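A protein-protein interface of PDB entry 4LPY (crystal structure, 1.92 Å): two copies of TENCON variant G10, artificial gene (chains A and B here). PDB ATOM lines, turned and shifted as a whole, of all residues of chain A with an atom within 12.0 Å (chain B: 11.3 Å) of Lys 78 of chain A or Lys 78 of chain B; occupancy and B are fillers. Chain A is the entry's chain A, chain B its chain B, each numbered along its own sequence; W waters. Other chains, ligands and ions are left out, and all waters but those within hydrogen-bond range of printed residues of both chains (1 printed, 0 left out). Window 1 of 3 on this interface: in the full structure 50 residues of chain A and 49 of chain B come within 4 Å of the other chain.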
ATOM      1  N   PRO A   3     -16.162  17.237  22.734  1.00  0.00           N
ATOM      2  CA  PRO A   3     -14.946  16.537  22.303  1.00  0.00           C
ATOM      3  C   PRO A   3     -14.257  17.212  21.115  1.00  0.00           C
ATOM      4  O   PRO A   3     -14.909  17.879  20.302  1.00  0.00           O
ATOM      5  CB  PRO A   3     -15.461  15.153  21.896  1.00  0.00           C
ATOM      6  CG  PRO A   3     -16.753  14.997  22.617  1.00  0.00           C
ATOM      7  CD  PRO A   3     -17.348  16.368  22.631  1.00  0.00           C
ATOM      8  N   ALA A  27     -13.583   6.247  20.487  1.00  0.00           N
ATOM      9  CA  ALA A  27     -14.852   6.291  19.727  1.00  0.00           C
ATOM     10  C   ALA A  27     -15.719   7.571  19.830  1.00  0.00           C
ATOM     11  O   ALA A  27     -16.934   7.515  19.637  1.00  0.00           O
ATOM     12  CB  ALA A  27     -15.693   5.021  19.985  1.00  0.00           C
ATOM     13  N   ALA A  28     -15.109   8.718  20.129  1.00  0.00           N
ATOM     14  CA  ALA A  28     -15.828   9.991  20.027  1.00  0.00           C
ATOM     15  C   ALA A  28     -16.135  10.303  18.560  1.00  0.00           C
ATOM     16  O   ALA A  28     -17.191  10.856  18.239  1.00  0.00           O
ATOM     17  CB  ALA A  28     -15.032  11.125  20.661  1.00  0.00           C
ATOM     18  N   PHE A  29     -15.209   9.942  17.675  1.00  0.00           N
ATOM     19  CA  PHE A  29     -15.304  10.338  16.267  1.00  0.00           C
ATOM     20  C   PHE A  29     -15.274   9.140  15.346  1.00  0.00           C
ATOM     21  O   PHE A  29     -14.534   8.172  15.581  1.00  0.00           O
ATOM     22  CB  PHE A  29     -14.194  11.335  15.894  1.00  0.00           C
ATOM     23  CG  PHE A  29     -14.149  12.551  16.780  1.00  0.00           C
ATOM     24  CD1 PHE A  29     -15.216  13.455  16.805  1.00  0.00           C
ATOM     25  CD2 PHE A  29     -13.047  12.796  17.588  1.00  0.00           C
ATOM     26  CE1 PHE A  29     -15.182  14.594  17.630  1.00  0.00           C
ATOM     27  CE2 PHE A  29     -12.997  13.928  18.417  1.00  0.00           C
ATOM     28  CZ  PHE A  29     -14.067  14.829  18.436  1.00  0.00           C
ATOM     29  N   ASP A  30     -16.088   9.220  14.295  1.00  0.00           N
ATOM     30  CA  ASP A  30     -16.168   8.181  13.268  1.00  0.00           C
ATOM     31  C   ASP A  30     -15.038   8.299  12.264  1.00  0.00           C
ATOM     32  O   ASP A  30     -14.594   7.300  11.691  1.00  0.00           O
ATOM     33  CB  ASP A  30     -17.514   8.277  12.536  1.00  0.00           C
ATOM     34  CG  ASP A  30     -18.691   8.007  13.460  1.00  0.00           C
ATOM     35  OD1 ASP A  30     -18.943   6.828  13.772  1.00  0.00           O
ATOM     36  OD2 ASP A  30     -19.358   8.974  13.871  1.00  0.00           O
ATOM     37  N   SER A  31     -14.575   9.529  12.052  1.00  0.00           N
ATOM     38  CA  SER A  31     -13.442   9.784  11.172  1.00  0.00           C
ATOM     39  C   SER A  31     -12.773  11.087  11.582  1.00  0.00           C
ATOM     40  O   SER A  31     -13.264  11.788  12.480  1.00  0.00           O
ATOM     41  CB  SER A  31     -13.884   9.807   9.701  1.00  0.00           C
ATOM     42  OG  SER A  31     -14.930  10.728   9.504  1.00  0.00           O
ATOM     43  N   GLY A  74     -12.473  16.387  14.322  1.00  0.00           N
ATOM     44  CA  GLY A  74     -13.143  15.113  14.583  1.00  0.00           C
ATOM     45  C   GLY A  74     -14.468  15.157  13.838  1.00  0.00           C
ATOM     46  O   GLY A  74     -15.144  16.192  13.860  1.00  0.00           O
ATOM     47  N   VAL A  75     -14.840  14.055  13.186  1.00  0.00           N
ATOM     48  CA  VAL A  75     -16.124  13.989  12.462  1.00  0.00           C
ATOM     49  C   VAL A  75     -17.022  12.932  13.106  1.00  0.00           C
ATOM     50  O   VAL A  75     -16.606  11.785  13.316  1.00  0.00           O
ATOM     51  CB  VAL A  75     -15.932  13.688  10.943  1.00  0.00           C
ATOM     52  CG1 VAL A  75     -17.283  13.485  10.228  1.00  0.00           C
ATOM     53  CG2 VAL A  75     -15.125  14.795  10.264  1.00  0.00           C
ATOM     54  N   PHE A  76     -18.253  13.315  13.423  1.00  0.00           N
ATOM     55  CA  PHE A  76     -19.167  12.364  14.050  1.00  0.00           C
ATOM     56  C   PHE A  76     -20.537  12.324  13.386  1.00  0.00           C
ATOM     57  O   PHE A  76     -21.070  13.354  12.962  1.00  0.00           O
ATOM     58  CB  PHE A  76     -19.247  12.556  15.581  1.00  0.00           C
ATOM     59  CG  PHE A  76     -19.587  13.955  16.019  1.00  0.00           C
ATOM     60  CD1 PHE A  76     -18.630  14.969  15.988  1.00  0.00           C
ATOM     61  CD2 PHE A  76     -20.868  14.259  16.467  1.00  0.00           C
ATOM     62  CE1 PHE A  76     -18.941  16.261  16.393  1.00  0.00           C
ATOM     63  CE2 PHE A  76     -21.193  15.553  16.877  1.00  0.00           C
ATOM     64  CZ  PHE A  76     -20.228  16.558  16.841  1.00  0.00           C
ATOM     65  N   MET A  77     -21.082  11.113  13.308  1.00  0.00           N
ATOM     66  CA  MET A  77     -22.430  10.851  12.806  1.00  0.00           C
ATOM     67  C   MET A  77     -23.366  10.587  13.976  1.00  0.00           C
ATOM     68  O   MET A  77     -23.013   9.847  14.902  1.00  0.00           O
ATOM     69  CB  MET A  77     -22.435   9.606  11.914  1.00  0.00           C
ATOM     70  CG  MET A  77     -21.980   9.825  10.489  1.00  0.00           C
ATOM     71  SD  MET A  77     -21.908   8.287   9.533  1.00  0.00           S
ATOM     72  CE  MET A  77     -20.245   7.704   9.877  1.00  0.00           C
ATOM     73  N   LYS A  78     -24.554  11.188  13.937  1.00  0.00           N
ATOM     74  CA  LYS A  78     -25.579  10.914  14.939  1.00  0.00           C
ATOM     75  C   LYS A  78     -26.867  10.494  14.244  1.00  0.00           C
ATOM     76  O   LYS A  78     -27.307  11.148  13.295  1.00  0.00           O
ATOM     77  CB  LYS A  78     -25.815  12.133  15.826  1.00  0.00           C
ATOM     78  N   MET A  79     -27.463   9.404  14.721  1.00  0.00           N
ATOM     79  CA  MET A  79     -28.766   8.955  14.232  1.00  0.00           C
ATOM     80  C   MET A  79     -29.826   9.221  15.292  1.00  0.00           C
ATOM     81  O   MET A  79     -29.624   8.908  16.471  1.00  0.00           O
ATOM     82  CB  MET A  79     -28.737   7.471  13.851  1.00  0.00           C
ATOM     83  CG  MET A  79     -27.557   7.103  12.957  1.00  0.00           C
ATOM     84  SD  MET A  79     -27.881   5.747  11.822  1.00  0.00           S
ATOM     85  CE  MET A  79     -26.296   5.610  10.990  1.00  0.00           C
ATOM     86  N   SER A  80     -30.948   9.800  14.864  1.00  0.00           N
ATOM     87  CA  SER A  80     -32.086  10.059  15.739  1.00  0.00           C
ATOM     88  C   SER A  80     -33.396   9.744  15.011  1.00  0.00           C
ATOM     89  O   SER A  80     -33.405   9.539  13.792  1.00  0.00           O
ATOM     90  CB  SER A  80     -32.075  11.511  16.210  1.00  0.00           C
ATOM     91  OG  SER A  80     -32.173  12.395  15.112  1.00  0.00           O
ATOM     92  N   LEU A  81     -34.497   9.706  15.757  1.00  0.00           N
ATOM     93  CA  LEU A  81     -35.815   9.544  15.148  1.00  0.00           C
ATOM     94  C   LEU A  81     -36.648  10.787  15.390  1.00  0.00           C
ATOM     95  O   LEU A  81     -36.766  11.251  16.523  1.00  0.00           O
ATOM     96  CB  LEU A  81     -36.531   8.294  15.676  1.00  0.00           C
ATOM     97  CG  LEU A  81     -35.916   6.931  15.335  1.00  0.00           C
ATOM     98  CD1 LEU A  81     -36.591   5.810  16.127  1.00  0.00           C
ATOM     99  CD2 LEU A  81     -35.989   6.637  13.842  1.00  0.00           C
ATOM    100  N   SER A  82     -37.221  11.321  14.317  1.00  0.00           N
ATOM    101  CA  SER A  82     -38.193  12.394  14.426  1.00  0.00           C
ATOM    102  C   SER A  82     -39.586  11.847  14.109  1.00  0.00           C
ATOM    103  O   SER A  82     -39.730  10.782  13.509  1.00  0.00           O
ATOM    104  CB  SER A  82     -37.846  13.556  13.497  1.00  0.00           C
ATOM    105  OG  SER A  82     -36.647  14.185  13.907  1.00  0.00           O
ATOM    106  N   LYS A  83     -40.593  12.598  14.525  1.00  0.00           N
ATOM    107  CA  LYS A  83     -41.975  12.178  14.500  1.00  0.00           C
ATOM    108  C   LYS A  83     -42.751  13.305  13.841  1.00  0.00           C
ATOM    109  O   LYS A  83     -42.535  14.470  14.176  1.00  0.00           O
ATOM    110  CB  LYS A  83     -42.435  12.089  15.943  1.00  0.00           C
ATOM    111  CG  LYS A  83     -43.032  10.809  16.388  1.00  0.00           C
ATOM    112  CD  LYS A  83     -43.069  10.849  17.905  1.00  0.00           C
ATOM    113  CE  LYS A  83     -44.318  10.224  18.460  1.00  0.00           C
ATOM    114  NZ  LYS A  83     -44.508  10.557  19.901  1.00  0.00           N
ATOM    115  N   SER A  84     -43.647  12.975  12.913  1.00  0.00           N
ATOM    116  CA  SER A  84     -44.597  13.949  12.367  1.00  0.00           C
ATOM    117  C   SER A  84     -45.618  14.335  13.436  1.00  0.00           C
ATOM    118  O   SER A  84     -45.688  13.700  14.503  1.00  0.00           O
ATOM    119  CB  SER A  84     -45.355  13.345  11.172  1.00  0.00           C
ATOM    120  OG  SER A  84     -46.438  12.528  11.623  1.00  0.00           O
ATOM    121  N   ALA B  27     -42.463   6.204   0.601  1.00  0.00           N
ATOM    122  CA  ALA B  27     -41.162   6.367   1.265  1.00  0.00           C
ATOM    123  C   ALA B  27     -40.969   7.668   2.057  1.00  0.00           C
ATOM    124  O   ALA B  27     -39.834   8.050   2.365  1.00  0.00           O
ATOM    125  CB  ALA B  27     -40.011   6.162   0.266  1.00  0.00           C
ATOM    126  N   ALA B  28     -42.060   8.353   2.389  1.00  0.00           N
ATOM    127  CA  ALA B  28     -41.954   9.533   3.238  1.00  0.00           C
ATOM    128  C   ALA B  28     -41.465   9.151   4.639  1.00  0.00           C
ATOM    129  O   ALA B  28     -40.711   9.906   5.267  1.00  0.00           O
ATOM    130  CB  ALA B  28     -43.277  10.269   3.315  1.00  0.00           C
ATOM    131  N   PHE B  29     -41.892   7.983   5.125  1.00  0.00           N
ATOM    132  CA  PHE B  29     -41.592   7.588   6.503  1.00  0.00           C
ATOM    133  C   PHE B  29     -40.906   6.237   6.589  1.00  0.00           C
ATOM    134  O   PHE B  29     -41.190   5.325   5.802  1.00  0.00           O
ATOM    135  CB  PHE B  29     -42.863   7.615   7.365  1.00  0.00           C
ATOM    136  CG  PHE B  29     -43.539   8.957   7.387  1.00  0.00           C
ATOM    137  CD1 PHE B  29     -42.973  10.029   8.097  1.00  0.00           C
ATOM    138  CD2 PHE B  29     -44.732   9.155   6.704  1.00  0.00           C
ATOM    139  CE1 PHE B  29     -43.591  11.278   8.125  1.00  0.00           C
ATOM    140  CE2 PHE B  29     -45.363  10.405   6.723  1.00  0.00           C
ATOM    141  CZ  PHE B  29     -44.785  11.467   7.438  1.00  0.00           C
ATOM    142  N   ASP B  30     -40.000   6.119   7.554  1.00  0.00           N
ATOM    143  CA  ASP B  30     -39.312   4.858   7.809  1.00  0.00           C
ATOM    144  C   ASP B  30     -40.171   3.887   8.624  1.00  0.00           C
ATOM    145  O   ASP B  30     -40.031   2.672   8.506  1.00  0.00           O
ATOM    146  CB  ASP B  30     -37.967   5.128   8.485  1.00  0.00           C
ATOM    147  CG  ASP B  30     -37.011   5.866   7.570  1.00  0.00           C
ATOM    148  OD1 ASP B  30     -36.757   5.352   6.464  1.00  0.00           O
ATOM    149  OD2 ASP B  30     -36.525   6.949   7.952  1.00  0.00           O
ATOM    150  N   SER B  31     -41.059   4.433   9.451  1.00  0.00           N
ATOM    151  CA  SER B  31     -42.064   3.617  10.127  1.00  0.00           C
ATOM    152  C   SER B  31     -43.236   4.486  10.569  1.00  0.00           C
ATOM    153  O   SER B  31     -43.212   5.709  10.387  1.00  0.00           O
ATOM    154  CB  SER B  31     -41.447   2.885  11.323  1.00  0.00           C
ATOM    155  OG  SER B  31     -40.935   3.815  12.239  1.00  0.00           O
ATOM    156  N   GLY B  74     -46.134   9.638  11.609  1.00  0.00           N
ATOM    157  CA  GLY B  74     -45.088   9.201  10.685  1.00  0.00           C
ATOM    158  C   GLY B  74     -43.749   9.359  11.394  1.00  0.00           C
ATOM    159  O   GLY B  74     -43.507  10.370  12.043  1.00  0.00           O
ATOM    160  N   VAL B  75     -42.881   8.364  11.270  1.00  0.00           N
ATOM    161  CA  VAL B  75     -41.586   8.382  11.956  1.00  0.00           C
ATOM    162  C   VAL B  75     -40.491   8.349  10.905  1.00  0.00           C
ATOM    163  O   VAL B  75     -40.498   7.489  10.019  1.00  0.00           O
ATOM    164  CB  VAL B  75     -41.423   7.167  12.921  1.00  0.00           C
ATOM    165  CG1 VAL B  75     -40.025   7.124  13.538  1.00  0.00           C
ATOM    166  CG2 VAL B  75     -42.497   7.187  14.009  1.00  0.00           C
ATOM    167  N   PHE B  76     -39.549   9.281  10.996  1.00  0.00           N
ATOM    168  CA  PHE B  76     -38.408   9.237  10.078  1.00  0.00           C
ATOM    169  C   PHE B  76     -37.068   9.220  10.795  1.00  0.00           C
ATOM    170  O   PHE B  76     -36.885   9.893  11.812  1.00  0.00           O
ATOM    171  CB  PHE B  76     -38.487  10.306   8.970  1.00  0.00           C
ATOM    172  CG  PHE B  76     -38.801  11.700   9.455  1.00  0.00           C
ATOM    173  CD1 PHE B  76     -40.080  12.034   9.901  1.00  0.00           C
ATOM    174  CD2 PHE B  76     -37.813  12.682   9.462  1.00  0.00           C
ATOM    175  CE1 PHE B  76     -40.368  13.320  10.347  1.00  0.00           C
ATOM    176  CE2 PHE B  76     -38.089  13.974   9.906  1.00  0.00           C
ATOM    177  CZ  PHE B  76     -39.370  14.294  10.350  1.00  0.00           C
ATOM    178  N   MET B  77     -36.144   8.437  10.244  1.00  0.00           N
ATOM    179  CA  MET B  77     -34.795   8.295  10.782  1.00  0.00           C
ATOM    180  C   MET B  77     -33.940   9.412  10.210  1.00  0.00           C
ATOM    181  O   MET B  77     -33.780   9.510   8.990  1.00  0.00           O
ATOM    182  CB  MET B  77     -34.210   6.920  10.422  1.00  0.00           C
ATOM    183  N   LYS B  78     -33.396  10.247  11.095  1.00  0.00           N
ATOM    184  CA  LYS B  78     -32.577  11.386  10.691  1.00  0.00           C
ATOM    185  C   LYS B  78     -31.099  11.084  10.960  1.00  0.00           C
ATOM    186  O   LYS B  78     -30.736  10.658  12.067  1.00  0.00           O
ATOM    187  CB  LYS B  78     -33.022  12.654  11.414  1.00  0.00           C
ATOM    188  N   MET B  79     -30.260  11.306   9.947  1.00  0.00           N
ATOM    189  CA  MET B  79     -28.817  11.097  10.070  1.00  0.00           C
ATOM    190  C   MET B  79     -28.113  12.448  10.070  1.00  0.00           C
ATOM    191  O   MET B  79     -28.325  13.263   9.176  1.00  0.00           O
ATOM    192  CB  MET B  79     -28.290  10.247   8.919  1.00  0.00           C
ATOM    193  CG  MET B  79     -28.826   8.821   8.878  1.00  0.00           C
ATOM    194  SD  MET B  79     -28.258   7.932   7.417  1.00  0.00           S
ATOM    195  CE  MET B  79     -29.069   8.834   6.117  1.00  0.00           C
ATOM    196  N   SER B  80     -27.278  12.686  11.068  1.00  0.00           N
ATOM    197  CA  SER B  80     -26.571  13.950  11.164  1.00  0.00           C
ATOM    198  C   SER B  80     -25.085  13.709  10.991  1.00  0.00           C
ATOM    199  O   SER B  80     -24.563  12.680  11.419  1.00  0.00           O
ATOM    200  CB  SER B  80     -26.840  14.610  12.514  1.00  0.00           C
ATOM    201  OG  SER B  80     -26.446  15.965  12.478  1.00  0.00           O
ATOM    202  N   LEU B  81     -24.415  14.664  10.363  1.00  0.00           N
ATOM    203  CA  LEU B  81     -22.978  14.616  10.187  1.00  0.00           C
ATOM    204  C   LEU B  81     -22.428  15.959  10.661  1.00  0.00           C
ATOM    205  O   LEU B  81     -22.854  17.013  10.182  1.00  0.00           O
ATOM    206  CB  LEU B  81     -22.646  14.343   8.722  1.00  0.00           C
ATOM    207  CG  LEU B  81     -21.241  13.932   8.290  1.00  0.00           C
ATOM    208  CD1 LEU B  81     -20.714  12.794   9.136  1.00  0.00           C
ATOM    209  CD2 LEU B  81     -21.275  13.521   6.821  1.00  0.00           C
ATOM    210  N   SER B  82     -21.486  15.919  11.600  1.00  0.00           N
ATOM    211  CA  SER B  82     -20.993  17.129  12.263  1.00  0.00           C
ATOM    212  C   SER B  82     -19.489  17.029  12.449  1.00  0.00           C
ATOM    213  O   SER B  82     -18.931  15.928  12.427  1.00  0.00           O
ATOM    214  CB  SER B  82     -21.655  17.306  13.630  1.00  0.00           C
ATOM    215  OG  SER B  82     -23.057  17.393  13.502  1.00  0.00           O
ATOM    216  N   LYS B  83     -18.837  18.175  12.631  1.00  0.00           N
ATOM    217  CA  LYS B  83     -17.400  18.178  12.941  1.00  0.00           C
ATOM    218  C   LYS B  83     -17.099  18.984  14.196  1.00  0.00           C
ATOM    219  O   LYS B  83     -17.806  19.946  14.526  1.00  0.00           O
ATOM    220  CB  LYS B  83     -16.570  18.674  11.748  1.00  0.00           C
ATOM    221  CG  LYS B  83     -16.714  20.183  11.434  1.00  0.00           C
ATOM    222  CD  LYS B  83     -15.998  20.532  10.125  1.00  0.00           C
ATOM    223  CE  LYS B  83     -15.891  22.042   9.899  1.00  0.00           C
ATOM    224  NZ  LYS B  83     -17.146  22.802  10.223  1.00  0.00           N
HETATM  225  O   HOH W   1     -23.748  14.644  14.133  1.00  0.00           O
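The backbone carbonyl oxygen of Ser 82 of chain B lies within hydrogen-bond range of the backbone NH of Phe 76 of chain A, at 2.9 Å. The backbone carbonyl oxygen (O) of Lys 78 of chain A sits at hydrogen-bond distance from the backbone NH (N) of Ser 80 of chain B (2.7 Å). The backbone NH (N) of Lys 78 of chain B is in hydrogen-bond range of the backbone carbonyl oxygen (O) of Ser 80 of chain A, at 2.8 Å. O of Phe 76 of chain B lies within hydrogen-bond range of N of Ser 82 of chain A, at 2.9 Å. N of Ser 84 of chain A sits at hydrogen-bond distance from O of Gly 74 of chain B (2.8 Å).
Gly 74 of chain A touches Lys 83 of chain B. CD1 of Leu 81 of chain B touches CG1 of Val 75 of chain A, at 3.7 Å. C of Lys 83 of chain B touches CE1 of Phe 76 of chain A, 3.95 Å away. Ser 80 of chain B touches Met 77 of chain A. Leu 81 of chain B touches Met 77 of chain A (CD1 to CG, 3.5 Å). Lys 78 of chain A touches Lys 78 of chain B. O of Lys 78 of chain A touches CA of Met 79 of chain B, at 3.6 Å. O of Ser 80 of chain A touches CA of Met 77 of chain B (3.5 Å). CA of Met 77 of chain B touches CD2 of Leu 81 of chain A, 3.7 Å away. Gly 74 of chain B touches Lys 83 of chain A.
Hydrophobic or aromatic side chains of chain B that line the printed part of chain A: Val 75, Phe 76, Met 77 and Leu 81. Along chain B the printed residues that touch a printed residue of chain A span positions 74 to 83. Of the 17 printed residues of chain A, 11 touch a printed residue of chain B. Printed residues of chain A that touch a printed residue of chain B: Gly 74, Val 75, Phe 76, Met 77, Lys 78, Met 79, Ser 80, Leu 81, Ser 82, Lys 83 and Ser 84. Hydrophobic or aromatic side chains of chain A that line the printed part of chain B: Val 75, Phe 76, Met 77 and Leu 81. Among the printed residues, no Asp or Glu carboxylate lies within 4 Å of a Lys or Arg side-chain nitrogen of the other chain.
Water W1 lies within hydrogen-bond range of the side-chain hydroxyl (OG) of Ser 82 of chain B (2.9 Å), the backbone carbonyl oxygen (O) of Phe 76 of chain A (3.2 Å) and the side-chain hydroxyl (OG) of Ser 80 of chain B (3.4 Å).
Ser 31 of chain A touches none of the printed residues of chain B. Of chain B, only Ser 80 (3.1 Å) and Leu 81 (3.5 Å) come within 4 Å of Met 77 of chain A. Lys 78 of chain A touches three residues of chain B. Met 79 of chain A touches just one residue of chain B: Lys 78. Of chain B, only Val 75 (3.4 Å) and Phe 76 (2.9 Å) come within 4 Å of Ser 82 of chain A. Of the printed residues of chain B, Lys 83 of chain A touches Gly 74. Of the printed residues of chain B, Ser 84 of chain A touches Gly 74. Ala 27 of chain B touches none of the printed residues of chain A. Of the printed residues of chain A, Gly 74 of chain B touches Lys 83 (3.4 Å) and Ser 84 (2.8 Å). Printed residues of chain A within 4 Å of Phe 76 of chain B: Leu 81 (3.5 Å) and Ser 82 (2.9 Å). Of chain A, only Ser 80 and Leu 81 come within 4 Å of Met 77 of chain B. Of the printed residues of chain A, Lys 78 of chain B touches Lys 78, Met 79 and Ser 80. Of chain A, only Lys 78 (3.6 Å) comes within 4 Å of Met 79 of chain B. Of chain A, only Phe 76, Met 77 and Lys 78 come within 4 Å of Ser 80 of chain B. Of chain A, only Val 75 (3.4 Å) and Phe 76 (2.9 Å) come within 4 Å of Ser 82 of chain B. Of the printed residues of chain A, Lys 83 of chain B touches Gly 74 (3.1 Å) and Phe 76 (3.95 Å). The nearest residue of chain B that does not touch Lys 78 of chain A is Leu 81 of chain B (5.0 Å). The nearest residue of chain A that does not touch Lys 78 of chain B is Ser 82 of chain A (4.7 Å). The nearest printed residue of chain B that does not touch Phe 76 of chain A is Met 79 of chain B (7.7 Å).
Phe 76 of chain A touches Leu 81 of chain B, and with the chains exchanged Leu 81 of chain A touches Phe 76 of chain B. Phe 76 of chain A touches Ser 82 of chain B, and with the chains exchanged Ser 82 of chain A touches Phe 76 of chain B. Met 77 of chain A touches Leu 81 of chain B, and with the chains exchanged Leu 81 of chain A touches Met 77 of chain B. Lys 78 of chain A touches its own counterpart, Lys 78 of chain B. Positions printed for both chains: 27, 28, 29, 30, 31, 74, 75, 76, 77, 78, 79, 80, 81, 82 and 83.
The backbone NH (N) of Asp 30 of chain A lies within hydrogen-bond range of the backbone carbonyl oxygen (O) of Val 75 of chain A (2.8 Å). N of Met 77 of chain A sits at hydrogen-bond distance from OD2 of Asp 30 of chain A. The backbone carbonyl oxygen of Ser 31 of chain A sits at hydrogen-bond distance from the backbone NH of Val 75 of chain A (2.8 Å). O of Val 75 of chain B lies within hydrogen-bond range of N of Asp 30 of chain B. OD2 of Asp 30 of chain B lies within hydrogen-bond range of N of Met 77 of chain B, 2.8 Å away. The backbone NH of Val 75 of chain B lies within hydrogen-bond range of the backbone carbonyl oxygen of Ser 31 of chain B.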
